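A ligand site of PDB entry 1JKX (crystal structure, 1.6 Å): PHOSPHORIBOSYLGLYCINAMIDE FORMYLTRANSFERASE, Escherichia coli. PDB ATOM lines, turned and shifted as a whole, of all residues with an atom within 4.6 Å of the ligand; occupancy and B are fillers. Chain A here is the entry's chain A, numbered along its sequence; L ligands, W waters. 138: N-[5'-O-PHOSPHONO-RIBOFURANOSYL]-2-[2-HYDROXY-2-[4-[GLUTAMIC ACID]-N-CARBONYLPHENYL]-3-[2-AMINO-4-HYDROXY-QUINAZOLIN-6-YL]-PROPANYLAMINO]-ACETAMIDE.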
ATOM      1  N   GLY A   9       5.244 -30.865 -11.986  1.00  0.00           N
ATOM      2  CA  GLY A   9       4.581 -32.010 -12.581  1.00  0.00           C
ATOM      3  C   GLY A   9       3.924 -33.080 -11.722  1.00  0.00           C
ATOM      4  O   GLY A   9       3.109 -32.794 -10.851  1.00  0.00           O
ATOM      5  N   ASN A  10       4.295 -34.321 -11.990  1.00  0.00           N
ATOM      6  CA  ASN A  10       3.717 -35.475 -11.318  1.00  0.00           C
ATOM      7  C   ASN A  10       3.607 -35.378  -9.817  1.00  0.00           C
ATOM      8  O   ASN A  10       2.561 -35.686  -9.255  1.00  0.00           O
ATOM      9  CB  ASN A  10       4.471 -36.742 -11.682  1.00  0.00           C
ATOM     10  CG  ASN A  10       3.735 -37.998 -11.239  1.00  0.00           C
ATOM     11  OD1 ASN A  10       3.947 -38.509 -10.143  1.00  0.00           O
ATOM     12  ND2 ASN A  10       2.833 -38.485 -12.095  1.00  0.00           N
ATOM     13  N   GLY A  11       4.689 -34.992  -9.156  1.00  0.00           N
ATOM     14  CA  GLY A  11       4.632 -34.868  -7.711  1.00  0.00           C
ATOM     15  C   GLY A  11       4.925 -36.124  -6.890  1.00  0.00           C
ATOM     16  O   GLY A  11       4.534 -36.202  -5.728  1.00  0.00           O
ATOM     17  N   SER A  12       5.610 -37.108  -7.469  1.00  0.00           N
ATOM     18  CA  SER A  12       5.914 -38.317  -6.703  1.00  0.00           C
ATOM     19  C   SER A  12       6.862 -37.998  -5.543  1.00  0.00           C
ATOM     20  O   SER A  12       6.760 -38.622  -4.477  1.00  0.00           O
ATOM     21  CB  SER A  12       6.521 -39.415  -7.601  1.00  0.00           C
ATOM     22  OG  SER A  12       7.851 -39.146  -8.010  1.00  0.00           O
ATOM     23  N   ASN A  13       7.751 -37.019  -5.732  1.00  0.00           N
ATOM     24  CA  ASN A  13       8.668 -36.660  -4.643  1.00  0.00           C
ATOM     25  C   ASN A  13       7.873 -35.926  -3.580  1.00  0.00           C
ATOM     26  O   ASN A  13       8.059 -36.182  -2.385  1.00  0.00           O
ATOM     27  CB  ASN A  13       9.822 -35.807  -5.161  1.00  0.00           C
ATOM     28  CG  ASN A  13      10.980 -36.658  -5.637  1.00  0.00           C
ATOM     29  OD1 ASN A  13      11.759 -37.184  -4.839  1.00  0.00           O
ATOM     30  ND2 ASN A  13      11.088 -36.840  -6.943  1.00  0.00           N
ATOM     31  N   LEU A  14       6.997 -35.024  -4.018  1.00  0.00           N
ATOM     32  CA  LEU A  14       6.114 -34.304  -3.095  1.00  0.00           C
ATOM     33  C   LEU A  14       5.352 -35.340  -2.255  1.00  0.00           C
ATOM     34  O   LEU A  14       5.212 -35.194  -1.047  1.00  0.00           O
ATOM     35  CB  LEU A  14       5.125 -33.445  -3.871  1.00  0.00           C
ATOM     36  CG  LEU A  14       3.882 -33.037  -3.077  1.00  0.00           C
ATOM     37  CD1 LEU A  14       4.296 -32.137  -1.907  1.00  0.00           C
ATOM     38  CD2 LEU A  14       2.902 -32.304  -3.970  1.00  0.00           C
ATOM     39  N   ARG A  64      10.662 -11.950 -15.188  1.00  0.00           N
ATOM     40  CA  ARG A  64      11.033 -12.999 -14.250  1.00  0.00           C
ATOM     41  C   ARG A  64      11.094 -12.394 -12.852  1.00  0.00           C
ATOM     42  O   ARG A  64      10.804 -13.060 -11.850  1.00  0.00           O
ATOM     43  CB  ARG A  64      12.386 -13.611 -14.635  1.00  0.00           C
ATOM     44  CG  ARG A  64      12.431 -14.161 -16.065  1.00  0.00           C
ATOM     45  CD  ARG A  64      13.663 -15.042 -16.295  1.00  0.00           C
ATOM     46  NE  ARG A  64      13.563 -16.296 -15.543  1.00  0.00           N
ATOM     47  CZ  ARG A  64      13.171 -17.446 -16.068  1.00  0.00           C
ATOM     48  NH1 ARG A  64      12.833 -17.520 -17.358  1.00  0.00           N
ATOM     49  NH2 ARG A  64      13.075 -18.523 -15.313  1.00  0.00           N
ATOM     50  N   LEU A  85      12.339 -27.651  -3.557  1.00  0.00           N
ATOM     51  CA  LEU A  85      12.074 -27.734  -4.993  1.00  0.00           C
ATOM     52  C   LEU A  85      12.015 -29.231  -5.300  1.00  0.00           C
ATOM     53  O   LEU A  85      12.996 -29.958  -5.093  1.00  0.00           O
ATOM     54  CB  LEU A  85      13.196 -27.067  -5.798  1.00  0.00           C
ATOM     55  CG  LEU A  85      13.577 -25.629  -5.431  1.00  0.00           C
ATOM     56  CD1 LEU A  85      14.632 -25.142  -6.418  1.00  0.00           C
ATOM     57  CD2 LEU A  85      12.352 -24.730  -5.458  1.00  0.00           C
ATOM     58  N   ALA A  86      10.861 -29.696  -5.763  1.00  0.00           N
ATOM     59  CA  ALA A  86      10.679 -31.105  -6.069  1.00  0.00           C
ATOM     60  C   ALA A  86      10.107 -31.241  -7.468  1.00  0.00           C
ATOM     61  O   ALA A  86       8.906 -31.400  -7.662  1.00  0.00           O
ATOM     62  CB  ALA A  86       9.746 -31.747  -5.037  1.00  0.00           C
ATOM     63  N   GLY A  87      10.994 -31.149  -8.452  1.00  0.00           N
ATOM     64  CA  GLY A  87      10.564 -31.219  -9.829  1.00  0.00           C
ATOM     65  C   GLY A  87      10.098 -29.856 -10.327  1.00  0.00           C
ATOM     66  O   GLY A  87       9.307 -29.789 -11.268  1.00  0.00           O
ATOM     67  N   PHE A  88      10.567 -28.775  -9.695  1.00  0.00           N
ATOM     68  CA  PHE A  88      10.181 -27.436 -10.126  1.00  0.00           C
ATOM     69  C   PHE A  88      11.083 -27.109 -11.318  1.00  0.00           C
ATOM     70  O   PHE A  88      12.291 -26.976 -11.155  1.00  0.00           O
ATOM     71  CB  PHE A  88      10.394 -26.432  -9.000  1.00  0.00           C
ATOM     72  CG  PHE A  88       9.863 -25.070  -9.303  1.00  0.00           C
ATOM     73  CD1 PHE A  88       8.491 -24.860  -9.471  1.00  0.00           C
ATOM     74  CD2 PHE A  88      10.721 -23.985  -9.395  1.00  0.00           C
ATOM     75  CE1 PHE A  88       7.990 -23.579  -9.719  1.00  0.00           C
ATOM     76  CE2 PHE A  88      10.239 -22.710  -9.653  1.00  0.00           C
ATOM     77  CZ  PHE A  88       8.867 -22.499  -9.821  1.00  0.00           C
ATOM     78  N   MET A  89      10.490 -26.964 -12.495  1.00  0.00           N
ATOM     79  CA  MET A  89      11.261 -26.737 -13.719  1.00  0.00           C
ATOM     80  C   MET A  89      11.314 -25.302 -14.238  1.00  0.00           C
ATOM     81  O   MET A  89      11.189 -25.058 -15.441  1.00  0.00           O
ATOM     82  CB  MET A  89      10.755 -27.658 -14.821  1.00  0.00           C
ATOM     83  CG  MET A  89      10.688 -29.128 -14.417  1.00  0.00           C
ATOM     84  SD  MET A  89      12.261 -29.837 -13.845  1.00  0.00           S
ATOM     85  CE  MET A  89      13.037 -30.174 -15.414  1.00  0.00           C
ATOM     86  N   ARG A  90      11.521 -24.354 -13.329  1.00  0.00           N
ATOM     87  CA  ARG A  90      11.625 -22.957 -13.700  1.00  0.00           C
ATOM     88  C   ARG A  90      12.760 -22.353 -12.889  1.00  0.00           C
ATOM     89  O   ARG A  90      12.813 -22.501 -11.669  1.00  0.00           O
ATOM     90  CB  ARG A  90      10.320 -22.219 -13.377  1.00  0.00           C
ATOM     91  CG  ARG A  90      10.372 -20.745 -13.743  1.00  0.00           C
ATOM     92  CD  ARG A  90       9.161 -19.990 -13.231  1.00  0.00           C
ATOM     93  NE  ARG A  90       9.420 -18.565 -13.335  1.00  0.00           N
ATOM     94  CZ  ARG A  90       9.202 -17.835 -14.422  1.00  0.00           C
ATOM     95  NH1 ARG A  90       8.695 -18.388 -15.514  1.00  0.00           N
ATOM     96  NH2 ARG A  90       9.538 -16.549 -14.438  1.00  0.00           N
ATOM     97  N   ILE A  91      13.676 -21.679 -13.573  1.00  0.00           N
ATOM     98  CA  ILE A  91      14.819 -21.050 -12.918  1.00  0.00           C
ATOM     99  C   ILE A  91      14.351 -20.013 -11.900  1.00  0.00           C
ATOM    100  O   ILE A  91      13.468 -19.194 -12.185  1.00  0.00           O
ATOM    101  CB  ILE A  91      15.739 -20.344 -13.952  1.00  0.00           C
ATOM    102  CG1 ILE A  91      16.440 -21.385 -14.815  1.00  0.00           C
ATOM    103  CG2 ILE A  91      16.760 -19.453 -13.235  1.00  0.00           C
ATOM    104  CD1 ILE A  91      17.261 -20.782 -15.935  1.00  0.00           C
ATOM    105  N   LEU A  92      14.932 -20.054 -10.708  1.00  0.00           N
ATOM    106  CA  LEU A  92      14.603 -19.108  -9.650  1.00  0.00           C
ATOM    107  C   LEU A  92      15.683 -18.023  -9.671  1.00  0.00           C
ATOM    108  O   LEU A  92      16.865 -18.314  -9.734  1.00  0.00           O
ATOM    109  CB  LEU A  92      14.552 -19.828  -8.305  1.00  0.00           C
ATOM    110  CG  LEU A  92      13.414 -20.847  -8.257  1.00  0.00           C
ATOM    111  CD1 LEU A  92      13.714 -21.951  -7.262  1.00  0.00           C
ATOM    112  CD2 LEU A  92      12.113 -20.133  -7.900  1.00  0.00           C
ATOM    113  N   VAL A  97      16.735 -16.815  -4.469  1.00  0.00           N
ATOM    114  CA  VAL A  97      17.727 -17.644  -3.813  1.00  0.00           C
ATOM    115  C   VAL A  97      18.255 -16.990  -2.531  1.00  0.00           C
ATOM    116  O   VAL A  97      18.413 -17.647  -1.502  1.00  0.00           O
ATOM    117  CB  VAL A  97      18.895 -17.944  -4.760  1.00  0.00           C
ATOM    118  CG1 VAL A  97      19.976 -18.733  -4.042  1.00  0.00           C
ATOM    119  CG2 VAL A  97      18.380 -18.709  -5.973  1.00  0.00           C
ATOM    120  N   ASN A 106      16.946 -28.520  -3.213  1.00  0.00           N
ATOM    121  CA  ASN A 106      16.624 -28.973  -4.559  1.00  0.00           C
ATOM    122  C   ASN A 106      17.093 -30.400  -4.753  1.00  0.00           C
ATOM    123  O   ASN A 106      18.007 -30.858  -4.054  1.00  0.00           O
ATOM    124  CB  ASN A 106      17.314 -28.087  -5.607  1.00  0.00           C
ATOM    125  CG  ASN A 106      17.011 -28.526  -7.033  1.00  0.00           C
ATOM    126  OD1 ASN A 106      15.848 -28.672  -7.403  1.00  0.00           O
ATOM    127  ND2 ASN A 106      18.054 -28.720  -7.835  1.00  0.00           N
ATOM    128  N   ILE A 107      16.462 -31.118  -5.675  1.00  0.00           N
ATOM    129  CA  ILE A 107      16.884 -32.475  -5.979  1.00  0.00           C
ATOM    130  C   ILE A 107      17.152 -32.483  -7.481  1.00  0.00           C
ATOM    131  O   ILE A 107      16.335 -32.016  -8.277  1.00  0.00           O
ATOM    132  CB  ILE A 107      15.835 -33.552  -5.568  1.00  0.00           C
ATOM    133  CG1 ILE A 107      16.490 -34.941  -5.641  1.00  0.00           C
ATOM    134  CG2 ILE A 107      14.615 -33.506  -6.475  1.00  0.00           C
ATOM    135  CD1 ILE A 107      15.765 -36.016  -4.837  1.00  0.00           C
ATOM    136  N   HIS A 108      18.322 -32.987  -7.849  1.00  0.00           N
ATOM    137  CA  HIS A 108      18.738 -33.021  -9.236  1.00  0.00           C
ATOM    138  C   HIS A 108      19.021 -34.469  -9.621  1.00  0.00           C
ATOM    139  O   HIS A 108      19.843 -35.130  -8.988  1.00  0.00           O
ATOM    140  CB  HIS A 108      19.977 -32.155  -9.400  1.00  0.00           C
ATOM    141  CG  HIS A 108      20.455 -32.057 -10.816  1.00  0.00           C
ATOM    142  ND1 HIS A 108      19.841 -31.263 -11.746  1.00  0.00           N
ATOM    143  CD2 HIS A 108      21.453 -32.702 -11.456  1.00  0.00           C
ATOM    144  CE1 HIS A 108      20.440 -31.414 -12.916  1.00  0.00           C
ATOM    145  NE2 HIS A 108      21.420 -32.286 -12.754  1.00  0.00           N
ATOM    146  N   PRO A 109      18.366 -34.965 -10.668  1.00  0.00           N
ATOM    147  CA  PRO A 109      18.536 -36.347 -11.126  1.00  0.00           C
ATOM    148  C   PRO A 109      19.803 -36.715 -11.877  1.00  0.00           C
ATOM    149  O   PRO A 109      19.751 -37.175 -13.016  1.00  0.00           O
ATOM    150  CB  PRO A 109      17.268 -36.585 -11.938  1.00  0.00           C
ATOM    151  CG  PRO A 109      17.090 -35.257 -12.634  1.00  0.00           C
ATOM    152  CD  PRO A 109      17.411 -34.241 -11.529  1.00  0.00           C
ATOM    153  N   PRO A 116      24.719 -31.407 -15.072  1.00  0.00           N
ATOM    154  CA  PRO A 116      24.077 -30.390 -14.232  1.00  0.00           C
ATOM    155  C   PRO A 116      22.824 -29.749 -14.844  1.00  0.00           C
ATOM    156  O   PRO A 116      22.101 -29.028 -14.164  1.00  0.00           O
ATOM    157  CB  PRO A 116      25.191 -29.378 -14.005  1.00  0.00           C
ATOM    158  CG  PRO A 116      25.940 -29.429 -15.317  1.00  0.00           C
ATOM    159  CD  PRO A 116      26.016 -30.925 -15.598  1.00  0.00           C
ATOM    160  N   GLY A 117      22.576 -30.027 -16.124  1.00  0.00           N
ATOM    161  CA  GLY A 117      21.437 -29.441 -16.805  1.00  0.00           C
ATOM    162  C   GLY A 117      20.178 -30.287 -16.937  1.00  0.00           C
ATOM    163  O   GLY A 117      19.780 -30.980 -15.994  1.00  0.00           O
ATOM    164  N   LEU A 118      19.568 -30.234 -18.111  1.00  0.00           N
ATOM    165  CA  LEU A 118      18.336 -30.969 -18.396  1.00  0.00           C
ATOM    166  C   LEU A 118      18.616 -32.304 -19.081  1.00  0.00           C
ATOM    167  O   LEU A 118      19.754 -32.572 -19.479  1.00  0.00           O
ATOM    168  CB  LEU A 118      17.430 -30.134 -19.307  1.00  0.00           C
ATOM    169  CG  LEU A 118      17.210 -28.673 -18.901  1.00  0.00           C
ATOM    170  CD1 LEU A 118      16.398 -27.972 -19.983  1.00  0.00           C
ATOM    171  CD2 LEU A 118      16.505 -28.601 -17.558  1.00  0.00           C
ATOM    172  N   HIS A 137      20.706 -31.011  -2.908  1.00  0.00           N
ATOM    173  CA  HIS A 137      21.637 -29.972  -2.526  1.00  0.00           C
ATOM    174  C   HIS A 137      20.981 -28.697  -2.032  1.00  0.00           C
ATOM    175  O   HIS A 137      19.784 -28.479  -2.252  1.00  0.00           O
ATOM    176  CB  HIS A 137      22.560 -29.637  -3.714  1.00  0.00           C
ATOM    177  CG  HIS A 137      21.872 -28.944  -4.855  1.00  0.00           C
ATOM    178  ND1 HIS A 137      21.755 -27.567  -4.919  1.00  0.00           N
ATOM    179  CD2 HIS A 137      21.307 -29.432  -5.985  1.00  0.00           C
ATOM    180  CE1 HIS A 137      21.152 -27.234  -6.046  1.00  0.00           C
ATOM    181  NE2 HIS A 137      20.862 -28.343  -6.711  1.00  0.00           N
ATOM    182  N   VAL A 139      20.417 -24.858  -2.387  1.00  0.00           N
ATOM    183  CA  VAL A 139      20.486 -23.980  -3.553  1.00  0.00           C
ATOM    184  C   VAL A 139      21.118 -22.645  -3.147  1.00  0.00           C
ATOM    185  O   VAL A 139      20.638 -21.984  -2.238  1.00  0.00           O
ATOM    186  CB  VAL A 139      19.077 -23.698  -4.140  1.00  0.00           C
ATOM    187  CG1 VAL A 139      19.197 -22.849  -5.393  1.00  0.00           C
ATOM    188  CG2 VAL A 139      18.375 -25.013  -4.463  1.00  0.00           C
ATOM    189  N   GLY A 145      25.243 -24.186  -8.360  1.00  0.00           N
ATOM    190  CA  GLY A 145      23.949 -24.349  -7.727  1.00  0.00           C
ATOM    191  C   GLY A 145      23.942 -24.547  -6.217  1.00  0.00           C
ATOM    192  O   GLY A 145      22.889 -24.427  -5.590  1.00  0.00           O
ATOM    193  N   GLN A 170      14.158 -42.360  -9.408  1.00  0.00           N
ATOM    194  CA  GLN A 170      13.119 -41.780  -8.559  1.00  0.00           C
ATOM    195  C   GLN A 170      12.870 -42.571  -7.278  1.00  0.00           C
ATOM    196  O   GLN A 170      12.479 -42.000  -6.258  1.00  0.00           O
ATOM    197  CB  GLN A 170      11.827 -41.601  -9.362  1.00  0.00           C
ATOM    198  CG  GLN A 170      11.996 -40.602 -10.497  1.00  0.00           C
ATOM    199  CD  GLN A 170      10.671 -40.055 -10.992  1.00  0.00           C
ATOM    200  OE1 GLN A 170       9.764 -40.798 -11.342  1.00  0.00           O
ATOM    201  NE2 GLN A 170      10.560 -38.730 -11.024  1.00  0.00           N
ATOM    202  N   GLU A 173      15.243 -41.225  -4.973  1.00  0.00           N
ATOM    203  CA  GLU A 173      14.822 -39.880  -4.591  1.00  0.00           C
ATOM    204  C   GLU A 173      13.777 -39.900  -3.481  1.00  0.00           C
ATOM    205  O   GLU A 173      13.866 -39.122  -2.518  1.00  0.00           O
ATOM    206  CB  GLU A 173      14.264 -39.136  -5.804  1.00  0.00           C
ATOM    207  CG  GLU A 173      15.340 -38.830  -6.834  1.00  0.00           C
ATOM    208  CD  GLU A 173      14.827 -37.982  -7.982  1.00  0.00           C
ATOM    209  OE1 GLU A 173      15.653 -37.253  -8.572  1.00  0.00           O
ATOM    210  OE2 GLU A 173      13.618 -38.042  -8.290  1.00  0.00           O
HETATM  211  N1  138 L   1      16.910 -22.161  -9.654  1.00  0.00           N
HETATM  212  C2  138 L   1      18.164 -21.843  -9.084  1.00  0.00           C
HETATM  213  NA2 138 L   1      18.446 -20.477  -8.645  1.00  0.00           N
HETATM  214  N3  138 L   1      19.155 -22.841  -8.947  1.00  0.00           N
HETATM  215  C4  138 L   1      18.914 -24.178  -9.376  1.00  0.00           C
HETATM  216  O4  138 L   1      19.938 -25.135  -9.212  1.00  0.00           O
HETATM  217  C4A 138 L   1      17.660 -24.518  -9.954  1.00  0.00           C
HETATM  218  C8A 138 L   1      16.638 -23.493 -10.085  1.00  0.00           C
HETATM  219  C8  138 L   1      15.352 -23.811 -10.665  1.00  0.00           C
HETATM  220  C7  138 L   1      15.087 -25.148 -11.119  1.00  0.00           C
HETATM  221  C6  138 L   1      16.119 -26.172 -10.989  1.00  0.00           C
HETATM  222  C9  138 L   1      15.880 -27.624 -11.505  1.00  0.00           C
HETATM  223  C10 138 L   1      16.577 -27.894 -12.967  1.00  0.00           C
HETATM  224  OA2 138 L   1      18.010 -27.870 -12.877  1.00  0.00           O
HETATM  225  CA1 138 L   1      16.143 -29.274 -13.566  1.00  0.00           C
HETATM  226  C5  138 L   1      17.385 -25.854 -10.407  1.00  0.00           C
HETATM  227  C13 138 L   1      16.973 -25.737 -14.448  1.00  0.00           C
HETATM  228  C12 138 L   1      16.532 -24.766 -15.404  1.00  0.00           C
HETATM  229  C11 138 L   1      15.211 -24.875 -15.964  1.00  0.00           C
HETATM  230  C17 138 L   1      14.701 -23.867 -16.973  1.00  0.00           C
HETATM  231  O17 138 L   1      15.795 -23.276 -17.708  1.00  0.00           O
HETATM  232  C16 138 L   1      14.330 -25.932 -15.575  1.00  0.00           C
HETATM  233  C15 138 L   1      14.752 -26.903 -14.616  1.00  0.00           C
HETATM  234  C14 138 L   1      16.096 -26.817 -14.039  1.00  0.00           C
HETATM  235  N   138 L   1      13.429 -23.577 -17.127  1.00  0.00           N
HETATM  236  CA  138 L   1      13.043 -22.588 -18.118  1.00  0.00           C
HETATM  237  C   138 L   1      12.885 -21.218 -17.491  1.00  0.00           C
HETATM  238  O   138 L   1      12.530 -20.186 -18.390  1.00  0.00           O
HETATM  239  OT  138 L   1      13.068 -21.016 -16.272  1.00  0.00           O
HETATM  240  CB  138 L   1      11.708 -23.063 -18.809  1.00  0.00           C
HETATM  241  CG  138 L   1      11.760 -24.409 -19.620  1.00  0.00           C
HETATM  242  CD  138 L   1      10.496 -24.918 -20.315  1.00  0.00           C
HETATM  243  OE2 138 L   1      10.514 -25.177 -21.558  1.00  0.00           O
HETATM  244  OE1 138 L   1       9.473 -25.078 -19.618  1.00  0.00           O
HETATM  245  C24 138 L   1      12.468 -35.585 -10.174  1.00  0.00           C
HETATM  246  O24 138 L   1      12.910 -36.908 -10.550  1.00  0.00           O
HETATM  247  C23 138 L   1      13.584 -34.560 -10.011  1.00  0.00           C
HETATM  248  O23 138 L   1      14.850 -35.107  -9.737  1.00  0.00           O
HETATM  249  C22 138 L   1      13.570 -33.824 -11.311  1.00  0.00           C
HETATM  250  O26 138 L   1      12.185 -33.675 -11.517  1.00  0.00           O
HETATM  251  C25 138 L   1      11.554 -34.933 -11.203  1.00  0.00           C
HETATM  252  C27 138 L   1      10.191 -34.650 -10.595  1.00  0.00           C
HETATM  253  O28 138 L   1       9.516 -35.872 -10.294  1.00  0.00           O
HETATM  254  N21 138 L   1      14.136 -32.495 -11.255  1.00  0.00           N
HETATM  255  C20 138 L   1      14.981 -32.027 -12.151  1.00  0.00           C
HETATM  256  O20 138 L   1      15.050 -32.504 -13.300  1.00  0.00           O
HETATM  257  C19 138 L   1      15.877 -30.858 -11.706  1.00  0.00           C
HETATM  258  N18 138 L   1      16.886 -30.229 -12.613  1.00  0.00           N
HETATM  259  P29 138 L   1       8.122 -35.872  -9.608  1.00  0.00           P
HETATM  260  O30 138 L   1       8.552 -35.667  -8.121  1.00  0.00           O
HETATM  261  O31 138 L   1       7.423 -37.276  -9.852  1.00  0.00           O
HETATM  262  O32 138 L   1       7.266 -34.832 -10.089  1.00  0.00           O
HETATM  263  O   HOH W   1       7.451 -33.719  -6.679  1.00  0.00           O
HETATM  264  O   HOH W   2      13.460 -34.331 -14.834  1.00  0.00           O
HETATM  265  O   HOH W   3       7.404 -34.259 -12.743  1.00  0.00           O
HETATM  266  O   HOH W   4      18.541 -23.319 -17.705  1.00  0.00           O
HETATM  267  O   HOH W   5      19.794 -27.568 -14.896  1.00  0.00           O
HETATM  268  O   HOH W   6      19.024 -28.894 -10.650  1.00  0.00           O
HETATM  269  O   HOH W   7      10.053 -19.353 -18.741  1.00  0.00           O
HETATM  270  O   HOH W   8       7.130 -39.469 -11.446  1.00  0.00           O
HETATM  271  O   HOH W   9       7.186 -32.007  -9.947  1.00  0.00           O
HETATM  272  O   HOH W  10      13.659 -37.247 -13.318  1.00  0.00           O
HETATM  273  O   HOH W  11      21.230 -21.301  -8.105  1.00  0.00           O
HETATM  274  O   HOH W  12      13.762 -31.114  -8.732  1.00  0.00           O
HETATM  275  O   HOH W  13      20.864 -27.500  -9.629  1.00  0.00           O
HETATM  276  O   HOH W  14      10.846 -33.086 -14.345  1.00  0.00           O
HETATM  277  O   HOH W  15      17.216 -32.121 -15.229  1.00  0.00           O
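O31 of the ligand sits at hydrogen-bond distance from OG of Ser 12 (2.7 Å).
The backbone NH (N) of Asn 13 is in hydrogen-bond range of an oxygen (O30) of the ligand (2.9 Å).
NH2 of Arg 64 lies within salt-bridge range of OT of the ligand, at 2.7 Å.
ND2 of Asn 13 is in hydrogen-bond range of O30 of the ligand (3.0 Å).
The backbone NH (N) of Gly 11 lies within hydrogen-bond range of an oxygen (O32) of the ligand (2.7 Å).
The side-chain carboxylate (OE1) of Glu 173 sits at hydrogen-bond distance from an oxygen (O23) of the ligand (2.6 Å).
O of Met 89 sits at hydrogen-bond distance from N of the ligand (3.2 Å).
OT of the ligand lies within hydrogen-bond range of N of Ile 91.
NA2 of the ligand sits at hydrogen-bond distance from O of Leu 92 (2.9 Å).
A ring nitrogen (ND1) of His 108 lies within hydrogen-bond range of a nitrogen (N18) of the ligand, 3.2 Å away.
The backbone NH of Leu 92 is in hydrogen-bond range of a nitrogen (N1) of the ligand.
The side-chain amide nitrogen of Gln 170 is in hydrogen-bond range of an oxygen (O24) of the ligand, 3.0 Å away.
The backbone NH (N) of Ser 12 is in hydrogen-bond range of an oxygen (O31) of the ligand, 3.0 Å away.
The guanidinium group (NH2) of Arg 64 sits at hydrogen-bond distance from the backbone carbonyl oxygen (O) of Ile 91 (3.2 Å).
The side-chain carboxylate (OE2) of Glu 173 sits at hydrogen-bond distance from the side-chain amide nitrogen (ND2) of Asn 13 (3.1 Å).
N of His 137 lies within hydrogen-bond range of O of Asn 106, at 2.9 Å.
N of Ser 12 is in hydrogen-bond range of OD1 of Asn 10 (3.4 Å).
A ring nitrogen (ND1) of His 137 lies close to the backbone carbonyl oxygen of Gly 145 (3.4 Å).
Residues that only touch the ligand: Asn 10 (3.5 Å), Gly 87 (3.4 Å), Phe 88 (3.3 Å), Arg 90 (3.0 Å), Val 97 (3.2 Å), Asn 106 (3.9 Å), Ile 107 (3.6 Å), Pro 109 (3.2 Å), Leu 118 (3.8 Å), His 137 (3.99 Å) and Val 139 (3.6 Å).
Hydrophobic or aromatic side chains within 4 Å of the ligand: Met 89, Ile 91, Leu 92, Val 97, Ile 107, His 108, Pro 109, Leu 118, His 137 and Val 139.
Within 4 Å of the ligand: Asn 10, Gly 11, Ser 12, Asn 13, Arg 64, Gly 87, Phe 88, Met 89, Arg 90, Ile 91, Leu 92, Val 97, Asn 106, Ile 107, His 108, Pro 109, Leu 118, His 137, Val 139, Gln 170 and Glu 173.
Along chain A the residues within 4 Å of the ligand span positions 10 to 173.
The nearest printed residue that does not touch the ligand is Gly 9 (4.1 Å).
Water W13 lies within hydrogen-bond range of an oxygen (O4) of the ligand (2.6 Å) and a ring nitrogen (NE2) of His 137 (3.0 Å).
Water W6 lies within hydrogen-bond range of OA2 of the ligand (2.7 Å), ND1 of His 108 (2.7 Å) and ND2 of Asn 106 (3.0 Å).
Water W5 lies within hydrogen-bond range of OA2 of the ligand (2.7 Å) and O of Pro 116 (2.8 Å).
Water W8 lies within hydrogen-bond range of an oxygen (O31) of the ligand (2.7 Å) and the side-chain amide oxygen (OE1) of Gln 170 (3.0 Å).
Water W15 lies within hydrogen-bond range of O of Gly 117 and O20 of the ligand.
Water W14 lies within hydrogen-bond range of O26 of the ligand and SD of Met 89.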
